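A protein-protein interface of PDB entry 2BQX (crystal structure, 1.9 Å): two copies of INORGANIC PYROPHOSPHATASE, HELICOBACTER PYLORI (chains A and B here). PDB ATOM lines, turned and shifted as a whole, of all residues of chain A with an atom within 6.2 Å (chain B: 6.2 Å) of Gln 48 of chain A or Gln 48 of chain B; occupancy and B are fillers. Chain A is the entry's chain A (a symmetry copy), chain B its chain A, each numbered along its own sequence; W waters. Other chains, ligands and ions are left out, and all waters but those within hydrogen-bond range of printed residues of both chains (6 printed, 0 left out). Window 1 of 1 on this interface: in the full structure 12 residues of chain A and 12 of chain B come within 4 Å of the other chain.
Water W6 lies within hydrogen-bond range of O of Gln 48 of chain B (2.6 Å) and ND2 of Asn 49 of chain A (3.2 Å). Water W3 bridges the side-chain amide nitrogen (NE2) of Gln 48 of chain B and the backbone carbonyl oxygen (O) of Ala 47 of chain A. Water W4 lies within hydrogen-bond range of N of Ala 47 of chain A (2.7 Å), ND1 of His 135 of chain B (2.8 Å) and N of Phe 136 of chain B (3.5 Å).
NE2 of Gln 48 of chain B is in hydrogen-bond range of OG1 of Thr 139 of chain B (2.9 Å). NE2 of Gln 48 of chain A lies within hydrogen-bond range of OG1 of Thr 139 of chain A, 2.9 Å away. The side-chain hydroxyl (OG1) of Thr 139 of chain A lies within hydrogen-bond range of the backbone carbonyl oxygen (O) of His 135 of chain A (2.9 Å).
Gln 48 of chain B touches its own counterpart, Gln 48 of chain A. Gln 48 of chain A touches Asn 49 of chain B, and with the chains exchanged Asn 49 of chain A touches Gln 48 of chain B. Asn 49 of chain B touches its own counterpart, Asn 49 of chain A. Of the 14 pairs that touch across the chains among the printed residues, 14 have their exchanged pair printed and touching as well.
The backbone carbonyl oxygen (O) of Ala 47 of chain B sits at hydrogen-bond distance from the backbone NH (N) of Asn 49 of chain A (3.2 Å). The backbone carbonyl oxygen (O) of Ala 47 of chain A sits at hydrogen-bond distance from the backbone NH (N) of Asn 49 of chain B (3.2 Å). NE2 of His 135 of chain B is in hydrogen-bond range of OD2 of Asp 142 of chain A, 3.0 Å away. The side-chain carboxylate of Asp 142 of chain B sits at hydrogen-bond distance from a ring nitrogen (NE2) of His 135 of chain A. The side-chain amide oxygen (OD1) of Asn 49 of chain A lies close to the side-chain amide oxygen (OD1) of Asn 49 of chain B, 2.2 Å away.
Hydrophobic or aromatic side chains of chain A that line the printed part of chain B: Ala 47 and His 135. Hydrophobic or aromatic side chains of chain B that line the printed part of chain A: Ala 47 and His 135. Among the printed residues, 14 pairs touch across the chains. Among the printed residues, no Asp or Glu carboxylate lies within 4 Å of a Lys or Arg side-chain nitrogen of the other chain.
Gln 48 of chain A touches just these residues of chain B: Ala 47 (3.4 Å), Gln 48 (3.9 Å), Asn 49 (3.6 Å) and His 135 (3.7 Å). Tyr 50 of chain A touches none of the printed residues of chain B. Of the printed residues of chain B, His 135 of chain A touches Gln 48, Thr 139 and Asp 142. Printed residues of chain A within 4 Å of Ala 47 of chain B: Gln 48 and Asn 49. Gln 48 of chain B touches just these residues of chain A: Ala 47 (3.4 Å), Gln 48 (3.9 Å), Asn 49 (3.6 Å) and His 135 (3.7 Å). The nearest residue of chain B that does not touch Gln 48 of chain A is Thr 139 of chain B (5.8 Å). The nearest printed residue of chain A that does not touch Asn 49 of chain B is Gly 46 of chain A (5.9 Å).
CE1 of His 135 of chain B touches OE1 of Gln 48 of chain A, at 3.7 Å. Asn 49 of chain A touches Gln 48 of chain B (OD1 to C, 3.6 Å). OE1 of Gln 48 of chain B touches CE1 of His 135 of chain A, at 3.7 Å. NE2 of His 135 of chain A touches O of Thr 139 of chain B, at 3.6 Å. Thr 139 of chain A touches His 135 of chain B (O to NE2, 3.6 Å).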
ATOM      1  N   HIS A  24      -2.005  31.653  -3.213  1.00  0.00           N
ATOM      2  CA  HIS A  24      -0.634  31.160  -3.039  1.00  0.00           C
ATOM      3  C   HIS A  24       0.195  31.894  -1.991  1.00  0.00           C
ATOM      4  O   HIS A  24       1.275  31.433  -1.621  1.00  0.00           O
ATOM      5  CB  HIS A  24       0.139  31.175  -4.369  1.00  0.00           C
ATOM      6  CG  HIS A  24      -0.479  30.324  -5.435  1.00  0.00           C
ATOM      7  ND1 HIS A  24      -0.771  28.992  -5.242  1.00  0.00           N
ATOM      8  CD2 HIS A  24      -0.861  30.613  -6.702  1.00  0.00           C
ATOM      9  CE1 HIS A  24      -1.308  28.496  -6.342  1.00  0.00           C
ATOM     10  NE2 HIS A  24      -1.373  29.457  -7.243  1.00  0.00           N
ATOM     11  N   SER A  25      -0.294  33.030  -1.511  1.00  0.00           N
ATOM     12  CA  SER A  25       0.443  33.797  -0.514  1.00  0.00           C
ATOM     13  C   SER A  25       0.294  33.196   0.880  1.00  0.00           C
ATOM     14  O   SER A  25      -0.669  32.475   1.154  1.00  0.00           O
ATOM     15  CB  SER A  25      -0.054  35.249  -0.498  1.00  0.00           C
ATOM     16  OG  SER A  25       0.585  35.996   0.523  1.00  0.00           O
ATOM     17  N   ASN A  26       1.258  33.477   1.753  1.00  0.00           N
ATOM     18  CA  ASN A  26       1.189  33.008   3.135  1.00  0.00           C
ATOM     19  C   ASN A  26       1.052  34.249   4.024  1.00  0.00           C
ATOM     20  O   ASN A  26       1.243  34.186   5.233  1.00  0.00           O
ATOM     21  CB  ASN A  26       2.440  32.191   3.514  1.00  0.00           C
ATOM     22  CG  ASN A  26       3.719  33.014   3.502  1.00  0.00           C
ATOM     23  OD1 ASN A  26       3.796  34.059   2.853  1.00  0.00           O
ATOM     24  ND2 ASN A  26       4.741  32.530   4.215  1.00  0.00           N
ATOM     25  N   LEU A  44       1.277  33.127   7.964  1.00  0.00           N
ATOM     26  CA  LEU A  44       0.987  31.746   8.355  1.00  0.00           C
ATOM     27  C   LEU A  44       2.143  31.121   9.135  1.00  0.00           C
ATOM     28  O   LEU A  44       3.304  31.262   8.758  1.00  0.00           O
ATOM     29  CB  LEU A  44       0.683  30.906   7.110  1.00  0.00           C
ATOM     30  CG  LEU A  44      -0.562  31.288   6.302  1.00  0.00           C
ATOM     31  CD1 LEU A  44      -0.677  30.379   5.094  1.00  0.00           C
ATOM     32  CD2 LEU A  44      -1.812  31.159   7.180  1.00  0.00           C
ATOM     33  N   TYR A  45       1.814  30.438  10.225  1.00  0.00           N
ATOM     34  CA  TYR A  45       2.819  29.785  11.062  1.00  0.00           C
ATOM     35  C   TYR A  45       3.372  28.535  10.386  1.00  0.00           C
ATOM     36  O   TYR A  45       4.515  28.155  10.616  1.00  0.00           O
ATOM     37  CB  TYR A  45       2.211  29.365  12.400  1.00  0.00           C
ATOM     38  CG  TYR A  45       2.020  30.475  13.418  1.00  0.00           C
ATOM     39  CD1 TYR A  45       1.618  31.754  13.033  1.00  0.00           C
ATOM     40  CD2 TYR A  45       2.175  30.214  14.779  1.00  0.00           C
ATOM     41  CE1 TYR A  45       1.370  32.749  13.993  1.00  0.00           C
ATOM     42  CE2 TYR A  45       1.929  31.188  15.740  1.00  0.00           C
ATOM     43  CZ  TYR A  45       1.527  32.452  15.341  1.00  0.00           C
ATOM     44  OH  TYR A  45       1.271  33.411  16.297  1.00  0.00           O
ATOM     45  N   GLY A  46       2.545  27.899   9.562  1.00  0.00           N
ATOM     46  CA  GLY A  46       2.967  26.686   8.895  1.00  0.00           C
ATOM     47  C   GLY A  46       3.419  26.870   7.466  1.00  0.00           C
ATOM     48  O   GLY A  46       3.307  27.957   6.891  1.00  0.00           O
ATOM     49  N   ALA A  47       3.934  25.785   6.896  1.00  0.00           N
ATOM     50  CA  ALA A  47       4.417  25.777   5.519  1.00  0.00           C
ATOM     51  C   ALA A  47       3.206  25.585   4.621  1.00  0.00           C
ATOM     52  O   ALA A  47       3.029  24.532   4.010  1.00  0.00           O
ATOM     53  CB  ALA A  47       5.407  24.633   5.336  1.00  0.00           C
ATOM     54  N   GLN A  48       2.373  26.616   4.551  1.00  0.00           N
ATOM     55  CA  GLN A  48       1.153  26.567   3.763  1.00  0.00           C
ATOM     56  C   GLN A  48       0.956  27.832   2.946  1.00  0.00           C
ATOM     57  O   GLN A  48       1.707  28.792   3.082  1.00  0.00           O
ATOM     58  CB  GLN A  48      -0.049  26.372   4.692  1.00  0.00           C
ATOM     59  CG  GLN A  48      -0.076  25.021   5.394  1.00  0.00           C
ATOM     60  CD  GLN A  48      -1.086  24.974   6.526  1.00  0.00           C
ATOM     61  OE1 GLN A  48      -0.838  25.480   7.624  1.00  0.00           O
ATOM     62  NE2 GLN A  48      -2.237  24.372   6.260  1.00  0.00           N
ATOM     63  N   ASN A  49      -0.056  27.821   2.088  1.00  0.00           N
ATOM     64  CA  ASN A  49      -0.359  28.977   1.266  1.00  0.00           C
ATOM     65  C   ASN A  49      -1.841  28.966   0.952  1.00  0.00           C
ATOM     66  O   ASN A  49      -2.432  27.898   0.793  1.00  0.00           O
ATOM     67  CB  ASN A  49       0.478  28.957  -0.016  1.00  0.00           C
ATOM     68  CG  ASN A  49       0.740  27.554  -0.530  1.00  0.00           C
ATOM     69  OD1 ASN A  49       1.613  26.833  -0.026  1.00  0.00           O
ATOM     70  ND2 ASN A  49      -0.019  27.155  -1.540  1.00  0.00           N
ATOM     71  N   TYR A  50      -2.452  30.145   0.885  1.00  0.00           N
ATOM     72  CA  TYR A  50      -3.883  30.213   0.608  1.00  0.00           C
ATOM     73  C   TYR A  50      -4.237  29.575  -0.727  1.00  0.00           C
ATOM     74  O   TYR A  50      -3.681  29.924  -1.766  1.00  0.00           O
ATOM     75  CB  TYR A  50      -4.374  31.661   0.666  1.00  0.00           C
ATOM     76  CG  TYR A  50      -4.625  32.128   2.075  1.00  0.00           C
ATOM     77  CD1 TYR A  50      -3.575  32.508   2.907  1.00  0.00           C
ATOM     78  CD2 TYR A  50      -5.920  32.158   2.591  1.00  0.00           C
ATOM     79  CE1 TYR A  50      -3.815  32.910   4.222  1.00  0.00           C
ATOM     80  CE2 TYR A  50      -6.167  32.552   3.898  1.00  0.00           C
ATOM     81  CZ  TYR A  50      -5.113  32.928   4.707  1.00  0.00           C
ATOM     82  OH  TYR A  50      -5.364  33.329   6.002  1.00  0.00           O
ATOM     83  N   HIS A 135      -8.962  21.089   3.782  1.00  0.00           N
ATOM     84  CA  HIS A 135      -7.785  20.704   4.544  1.00  0.00           C
ATOM     85  C   HIS A 135      -6.964  21.927   4.966  1.00  0.00           C
ATOM     86  O   HIS A 135      -6.328  21.931   6.024  1.00  0.00           O
ATOM     87  CB  HIS A 135      -6.947  19.729   3.711  1.00  0.00           C
ATOM     88  CG  HIS A 135      -5.640  19.365   4.337  1.00  0.00           C
ATOM     89  ND1 HIS A 135      -4.460  19.999   4.014  1.00  0.00           N
ATOM     90  CD2 HIS A 135      -5.331  18.461   5.297  1.00  0.00           C
ATOM     91  CE1 HIS A 135      -3.481  19.503   4.750  1.00  0.00           C
ATOM     92  NE2 HIS A 135      -3.983  18.568   5.536  1.00  0.00           N
ATOM     93  N   PHE A 136      -6.984  22.969   4.143  1.00  0.00           N
ATOM     94  CA  PHE A 136      -6.251  24.186   4.470  1.00  0.00           C
ATOM     95  C   PHE A 136      -6.835  24.843   5.720  1.00  0.00           C
ATOM     96  O   PHE A 136      -6.115  25.167   6.669  1.00  0.00           O
ATOM     97  CB  PHE A 136      -6.312  25.186   3.316  1.00  0.00           C
ATOM     98  CG  PHE A 136      -5.730  26.526   3.655  1.00  0.00           C
ATOM     99  CD1 PHE A 136      -4.352  26.721   3.654  1.00  0.00           C
ATOM    100  CD2 PHE A 136      -6.559  27.588   4.002  1.00  0.00           C
ATOM    101  CE1 PHE A 136      -3.806  27.958   3.993  1.00  0.00           C
ATOM    102  CE2 PHE A 136      -6.024  28.830   4.344  1.00  0.00           C
ATOM    103  CZ  PHE A 136      -4.642  29.017   4.338  1.00  0.00           C
ATOM    104  N   PHE A 137      -8.145  25.040   5.723  1.00  0.00           N
ATOM    105  CA  PHE A 137      -8.783  25.674   6.872  1.00  0.00           C
ATOM    106  C   PHE A 137      -8.723  24.772   8.094  1.00  0.00           C
ATOM    107  O   PHE A 137      -8.627  25.245   9.229  1.00  0.00           O
ATOM    108  CB  PHE A 137     -10.227  26.042   6.520  1.00  0.00           C
ATOM    109  CG  PHE A 137     -10.328  27.243   5.626  1.00  0.00           C
ATOM    110  CD1 PHE A 137     -10.066  28.517   6.126  1.00  0.00           C
ATOM    111  CD2 PHE A 137     -10.632  27.102   4.277  1.00  0.00           C
ATOM    112  CE1 PHE A 137     -10.099  29.634   5.294  1.00  0.00           C
ATOM    113  CE2 PHE A 137     -10.668  28.212   3.436  1.00  0.00           C
ATOM    114  CZ  PHE A 137     -10.400  29.484   3.949  1.00  0.00           C
ATOM    115  N   THR A 139      -6.275  22.930   8.959  1.00  0.00           N
ATOM    116  CA  THR A 139      -4.937  22.893   9.549  1.00  0.00           C
ATOM    117  C   THR A 139      -4.109  24.176   9.629  1.00  0.00           C
ATOM    118  O   THR A 139      -3.124  24.220  10.362  1.00  0.00           O
ATOM    119  CB  THR A 139      -4.053  21.878   8.801  1.00  0.00           C
ATOM    120  OG1 THR A 139      -3.853  22.325   7.449  1.00  0.00           O
ATOM    121  CG2 THR A 139      -4.699  20.508   8.788  1.00  0.00           C
ATOM    122  N   TYR A 140      -4.495  25.214   8.897  1.00  0.00           N
ATOM    123  CA  TYR A 140      -3.702  26.438   8.869  1.00  0.00           C
ATOM    124  C   TYR A 140      -3.554  27.183  10.193  1.00  0.00           C
ATOM    125  O   TYR A 140      -2.687  28.049  10.327  1.00  0.00           O
ATOM    126  CB  TYR A 140      -4.218  27.371   7.764  1.00  0.00           C
ATOM    127  CG  TYR A 140      -5.376  28.278   8.124  1.00  0.00           C
ATOM    128  CD1 TYR A 140      -6.554  27.772   8.671  1.00  0.00           C
ATOM    129  CD2 TYR A 140      -5.313  29.645   7.846  1.00  0.00           C
ATOM    130  CE1 TYR A 140      -7.644  28.609   8.926  1.00  0.00           C
ATOM    131  CE2 TYR A 140      -6.394  30.487   8.095  1.00  0.00           C
ATOM    132  CZ  TYR A 140      -7.555  29.959   8.633  1.00  0.00           C
ATOM    133  OH  TYR A 140      -8.632  30.783   8.863  1.00  0.00           O
ATOM    134  N   LYS A 141      -4.387  26.846  11.169  1.00  0.00           N
ATOM    135  CA  LYS A 141      -4.293  27.479  12.478  1.00  0.00           C
ATOM    136  C   LYS A 141      -3.828  26.488  13.536  1.00  0.00           C
ATOM    137  O   LYS A 141      -3.842  26.799  14.725  1.00  0.00           O
ATOM    138  CB  LYS A 141      -5.634  28.093  12.889  1.00  0.00           C
ATOM    139  CG  LYS A 141      -5.942  29.402  12.198  1.00  0.00           C
ATOM    140  CD  LYS A 141      -7.214  30.017  12.739  1.00  0.00           C
ATOM    141  CE  LYS A 141      -7.455  31.378  12.132  1.00  0.00           C
ATOM    142  NZ  LYS A 141      -8.673  32.016  12.714  1.00  0.00           N
ATOM    143  N   ASP A 142      -3.408  25.300  13.109  1.00  0.00           N
ATOM    144  CA  ASP A 142      -2.935  24.291  14.062  1.00  0.00           C
ATOM    145  C   ASP A 142      -1.868  24.852  14.994  1.00  0.00           C
ATOM    146  O   ASP A 142      -1.961  24.703  16.209  1.00  0.00           O
ATOM    147  CB  ASP A 142      -2.333  23.067  13.351  1.00  0.00           C
ATOM    148  CG  ASP A 142      -3.379  22.152  12.720  1.00  0.00           C
ATOM    149  OD1 ASP A 142      -4.574  22.232  13.086  1.00  0.00           O
ATOM    150  OD2 ASP A 142      -2.982  21.330  11.861  1.00  0.00           O
ATOM    151  N   HIS B  24      10.161  25.604  -0.674  1.00  0.00           N
ATOM    152  CA  HIS B  24       8.950  26.312  -1.107  1.00  0.00           C
ATOM    153  C   HIS B  24       8.165  25.637  -2.226  1.00  0.00           C
ATOM    154  O   HIS B  24       7.037  26.031  -2.518  1.00  0.00           O
ATOM    155  CB  HIS B  24       9.270  27.754  -1.538  1.00  0.00           C
ATOM    156  CG  HIS B  24       9.875  28.587  -0.450  1.00  0.00           C
ATOM    157  ND1 HIS B  24       9.281  28.738   0.782  1.00  0.00           N
ATOM    158  CD2 HIS B  24      11.017  29.314  -0.410  1.00  0.00           C
ATOM    159  CE1 HIS B  24      10.031  29.519   1.539  1.00  0.00           C
ATOM    160  NE2 HIS B  24      11.090  29.883   0.839  1.00  0.00           N
ATOM    161  N   SER B  25       8.749  24.626  -2.857  1.00  0.00           N
ATOM    162  CA  SER B  25       8.069  23.935  -3.947  1.00  0.00           C
ATOM    163  C   SER B  25       7.029  22.949  -3.423  1.00  0.00           C
ATOM    164  O   SER B  25       7.112  22.496  -2.279  1.00  0.00           O
ATOM    165  CB  SER B  25       9.092  23.184  -4.810  1.00  0.00           C
ATOM    166  OG  SER B  25       8.449  22.432  -5.826  1.00  0.00           O
ATOM    167  N   ASN B  26       6.039  22.633  -4.255  1.00  0.00           N
ATOM    168  CA  ASN B  26       5.022  21.653  -3.886  1.00  0.00           C
ATOM    169  C   ASN B  26       5.191  20.455  -4.826  1.00  0.00           C
ATOM    170  O   ASN B  26       4.314  19.603  -4.931  1.00  0.00           O
ATOM    171  CB  ASN B  26       3.604  22.247  -3.995  1.00  0.00           C
ATOM    172  CG  ASN B  26       3.215  22.613  -5.419  1.00  0.00           C
ATOM    173  OD1 ASN B  26       4.073  22.816  -6.280  1.00  0.00           O
ATOM    174  ND2 ASN B  26       1.905  22.713  -5.668  1.00  0.00           N
ATOM    175  N   LEU B  44       2.131  17.795  -4.196  1.00  0.00           N
ATOM    176  CA  LEU B  44       1.394  17.805  -2.931  1.00  0.00           C
ATOM    177  C   LEU B  44      -0.109  17.966  -3.151  1.00  0.00           C
ATOM    178  O   LEU B  44      -0.543  18.796  -3.946  1.00  0.00           O
ATOM    179  CB  LEU B  44       1.914  18.934  -2.035  1.00  0.00           C
ATOM    180  CG  LEU B  44       3.370  18.833  -1.567  1.00  0.00           C
ATOM    181  CD1 LEU B  44       3.715  20.050  -0.730  1.00  0.00           C
ATOM    182  CD2 LEU B  44       3.565  17.555  -0.744  1.00  0.00           C
ATOM    183  N   TYR B  45      -0.896  17.161  -2.443  1.00  0.00           N
ATOM    184  CA  TYR B  45      -2.352  17.212  -2.552  1.00  0.00           C
ATOM    185  C   TYR B  45      -2.915  18.449  -1.861  1.00  0.00           C
ATOM    186  O   TYR B  45      -3.960  18.960  -2.250  1.00  0.00           O
ATOM    187  CB  TYR B  45      -2.981  15.982  -1.898  1.00  0.00           C
ATOM    188  CG  TYR B  45      -2.919  14.698  -2.704  1.00  0.00           C
ATOM    189  CD1 TYR B  45      -1.802  14.374  -3.473  1.00  0.00           C
ATOM    190  CD2 TYR B  45      -3.962  13.774  -2.634  1.00  0.00           C
ATOM    191  CE1 TYR B  45      -1.728  13.146  -4.153  1.00  0.00           C
ATOM    192  CE2 TYR B  45      -3.901  12.554  -3.297  1.00  0.00           C
ATOM    193  CZ  TYR B  45      -2.782  12.247  -4.054  1.00  0.00           C
ATOM    194  OH  TYR B  45      -2.719  11.030  -4.701  1.00  0.00           O
ATOM    195  N   GLY B  46      -2.217  18.913  -0.829  1.00  0.00           N
ATOM    196  CA  GLY B  46      -2.684  20.065  -0.089  1.00  0.00           C
ATOM    197  C   GLY B  46      -2.020  21.370  -0.459  1.00  0.00           C
ATOM    198  O   GLY B  46      -1.066  21.407  -1.242  1.00  0.00           O
ATOM    199  N   ALA B  47      -2.540  22.449   0.119  1.00  0.00           N
ATOM    200  CA  ALA B  47      -2.023  23.792  -0.118  1.00  0.00           C
ATOM    201  C   ALA B  47      -0.818  23.975   0.793  1.00  0.00           C
ATOM    202  O   ALA B  47      -0.864  24.731   1.760  1.00  0.00           O
ATOM    203  CB  ALA B  47      -3.102  24.817   0.210  1.00  0.00           C
ATOM    204  N   GLN B  48       0.258  23.269   0.470  1.00  0.00           N
ATOM    205  CA  GLN B  48       1.473  23.311   1.266  1.00  0.00           C
ATOM    206  C   GLN B  48       2.715  23.439   0.399  1.00  0.00           C
ATOM    207  O   GLN B  48       2.637  23.378  -0.822  1.00  0.00           O
ATOM    208  CB  GLN B  48       1.574  22.038   2.111  1.00  0.00           C
ATOM    209  CG  GLN B  48       0.500  21.919   3.184  1.00  0.00           C
ATOM    210  CD  GLN B  48       0.434  20.529   3.789  1.00  0.00           C
ATOM    211  OE1 GLN B  48      -0.130  19.603   3.199  1.00  0.00           O
ATOM    212  NE2 GLN B  48       1.017  20.373   4.970  1.00  0.00           N
ATOM    213  N   ASN B  49       3.858  23.626   1.044  1.00  0.00           N
ATOM    214  CA  ASN B  49       5.114  23.743   0.329  1.00  0.00           C
ATOM    215  C   ASN B  49       6.228  23.263   1.236  1.00  0.00           C
ATOM    216  O   ASN B  49       6.166  23.458   2.451  1.00  0.00           O
ATOM    217  CB  ASN B  49       5.347  25.190  -0.114  1.00  0.00           C
ATOM    218  CG  ASN B  49       4.795  26.206   0.870  1.00  0.00           C
ATOM    219  OD1 ASN B  49       3.586  26.479   0.905  1.00  0.00           O
ATOM    220  ND2 ASN B  49       5.679  26.771   1.676  1.00  0.00           N
ATOM    221  N   TYR B  50       7.237  22.615   0.662  1.00  0.00           N
ATOM    222  CA  TYR B  50       8.336  22.104   1.474  1.00  0.00           C
ATOM    223  C   TYR B  50       9.042  23.211   2.242  1.00  0.00           C
ATOM    224  O   TYR B  50       9.488  24.199   1.665  1.00  0.00           O
ATOM    225  CB  TYR B  50       9.329  21.324   0.608  1.00  0.00           C
ATOM    226  CG  TYR B  50       8.873  19.915   0.338  1.00  0.00           C
ATOM    227  CD1 TYR B  50       7.903  19.641  -0.623  1.00  0.00           C
ATOM    228  CD2 TYR B  50       9.392  18.849   1.074  1.00  0.00           C
ATOM    229  CE1 TYR B  50       7.465  18.335  -0.846  1.00  0.00           C
ATOM    230  CE2 TYR B  50       8.959  17.549   0.862  1.00  0.00           C
ATOM    231  CZ  TYR B  50       8.000  17.297  -0.098  1.00  0.00           C
ATOM    232  OH  TYR B  50       7.580  16.001  -0.311  1.00  0.00           O
ATOM    233  N   HIS B 135       5.099  20.129  11.709  1.00  0.00           N
ATOM    234  CA  HIS B 135       3.711  20.234  11.286  1.00  0.00           C
ATOM    235  C   HIS B 135       3.549  19.891   9.801  1.00  0.00           C
ATOM    236  O   HIS B 135       2.518  19.359   9.382  1.00  0.00           O
ATOM    237  CB  HIS B 135       3.201  21.646  11.592  1.00  0.00           C
ATOM    238  CG  HIS B 135       1.824  21.916  11.078  1.00  0.00           C
ATOM    239  ND1 HIS B 135       1.591  22.546   9.875  1.00  0.00           N
ATOM    240  CD2 HIS B 135       0.606  21.607  11.584  1.00  0.00           C
ATOM    241  CE1 HIS B 135       0.289  22.611   9.660  1.00  0.00           C
ATOM    242  NE2 HIS B 135      -0.331  22.049  10.682  1.00  0.00           N
ATOM    243  N   PHE B 136       4.572  20.187   9.008  1.00  0.00           N
ATOM    244  CA  PHE B 136       4.520  19.877   7.583  1.00  0.00           C
ATOM    245  C   PHE B 136       4.463  18.366   7.367  1.00  0.00           C
ATOM    246  O   PHE B 136       3.603  17.854   6.645  1.00  0.00           O
ATOM    247  CB  PHE B 136       5.745  20.432   6.860  1.00  0.00           C
ATOM    248  CG  PHE B 136       5.841  19.996   5.427  1.00  0.00           C
ATOM    249  CD1 PHE B 136       5.072  20.614   4.446  1.00  0.00           C
ATOM    250  CD2 PHE B 136       6.681  18.949   5.063  1.00  0.00           C
ATOM    251  CE1 PHE B 136       5.140  20.197   3.117  1.00  0.00           C
ATOM    252  CE2 PHE B 136       6.756  18.521   3.737  1.00  0.00           C
ATOM    253  CZ  PHE B 136       5.984  19.148   2.761  1.00  0.00           C
ATOM    254  N   PHE B 137       5.381  17.647   7.994  1.00  0.00           N
ATOM    255  CA  PHE B 137       5.409  16.197   7.831  1.00  0.00           C
ATOM    256  C   PHE B 137       4.191  15.554   8.475  1.00  0.00           C
ATOM    257  O   PHE B 137       3.685  14.534   8.001  1.00  0.00           O
ATOM    258  CB  PHE B 137       6.709  15.638   8.413  1.00  0.00           C
ATOM    259  CG  PHE B 137       7.905  15.897   7.543  1.00  0.00           C
ATOM    260  CD1 PHE B 137       8.072  15.196   6.351  1.00  0.00           C
ATOM    261  CD2 PHE B 137       8.834  16.872   7.884  1.00  0.00           C
ATOM    262  CE1 PHE B 137       9.145  15.467   5.505  1.00  0.00           C
ATOM    263  CE2 PHE B 137       9.911  17.152   7.046  1.00  0.00           C
ATOM    264  CZ  PHE B 137      10.067  16.445   5.851  1.00  0.00           C
ATOM    265  N   THR B 139       1.221  16.699   8.452  1.00  0.00           N
ATOM    266  CA  THR B 139       0.008  16.904   7.659  1.00  0.00           C
ATOM    267  C   THR B 139       0.077  16.817   6.134  1.00  0.00           C
ATOM    268  O   THR B 139      -0.960  16.704   5.485  1.00  0.00           O
ATOM    269  CB  THR B 139      -0.602  18.284   7.966  1.00  0.00           C
ATOM    270  OG1 THR B 139       0.304  19.313   7.535  1.00  0.00           O
ATOM    271  CG2 THR B 139      -0.868  18.437   9.450  1.00  0.00           C
ATOM    272  N   TYR B 140       1.273  16.861   5.560  1.00  0.00           N
ATOM    273  CA  TYR B 140       1.398  16.862   4.107  1.00  0.00           C
ATOM    274  C   TYR B 140       0.882  15.625   3.378  1.00  0.00           C
ATOM    275  O   TYR B 140       0.686  15.655   2.161  1.00  0.00           O
ATOM    276  CB  TYR B 140       2.847  17.174   3.707  1.00  0.00           C
ATOM    277  CG  TYR B 140       3.809  16.006   3.664  1.00  0.00           C
ATOM    278  CD1 TYR B 140       3.970  15.155   4.756  1.00  0.00           C
ATOM    279  CD2 TYR B 140       4.615  15.797   2.542  1.00  0.00           C
ATOM    280  CE1 TYR B 140       4.918  14.127   4.732  1.00  0.00           C
ATOM    281  CE2 TYR B 140       5.562  14.777   2.509  1.00  0.00           C
ATOM    282  CZ  TYR B 140       5.707  13.949   3.608  1.00  0.00           C
ATOM    283  OH  TYR B 140       6.655  12.953   3.587  1.00  0.00           O
ATOM    284  N   LYS B 141       0.652  14.545   4.114  1.00  0.00           N
ATOM    285  CA  LYS B 141       0.123  13.331   3.507  1.00  0.00           C
ATOM    286  C   LYS B 141      -1.294  13.050   3.986  1.00  0.00           C
ATOM    287  O   LYS B 141      -1.845  11.987   3.705  1.00  0.00           O
ATOM    288  CB  LYS B 141       1.024  12.128   3.806  1.00  0.00           C
ATOM    289  CG  LYS B 141       2.281  12.087   2.968  1.00  0.00           C
ATOM    290  CD  LYS B 141       3.061  10.815   3.220  1.00  0.00           C
ATOM    291  CE  LYS B 141       4.252  10.720   2.296  1.00  0.00           C
ATOM    292  NZ  LYS B 141       4.985   9.436   2.495  1.00  0.00           N
ATOM    293  N   ASP B 142      -1.892  14.001   4.698  1.00  0.00           N
ATOM    294  CA  ASP B 142      -3.260  13.815   5.190  1.00  0.00           C
ATOM    295  C   ASP B 142      -4.211  13.410   4.070  1.00  0.00           C
ATOM    296  O   ASP B 142      -4.955  12.442   4.204  1.00  0.00           O
ATOM    297  CB  ASP B 142      -3.820  15.096   5.833  1.00  0.00           C
ATOM    298  CG  ASP B 142      -3.238  15.391   7.212  1.00  0.00           C
ATOM    299  OD1 ASP B 142      -2.667  14.478   7.852  1.00  0.00           O
ATOM    300  OD2 ASP B 142      -3.380  16.553   7.661  1.00  0.00           O
HETATM  301  O   HOH W   1      -2.770  23.578   3.708  1.00  0.00           O
HETATM  302  O   HOH W   2      -4.515  21.956   1.952  1.00  0.00           O
HETATM  303  O   HOH W   3       2.488  22.419   6.009  1.00  0.00           O
HETATM  304  O   HOH W   4       3.832  23.506   8.412  1.00  0.00           O
HETATM  305  O   HOH W   5       4.237  29.132   3.210  1.00  0.00           O
HETATM  306  O   HOH W   6       1.139  24.415  -2.614  1.00  0.00           O
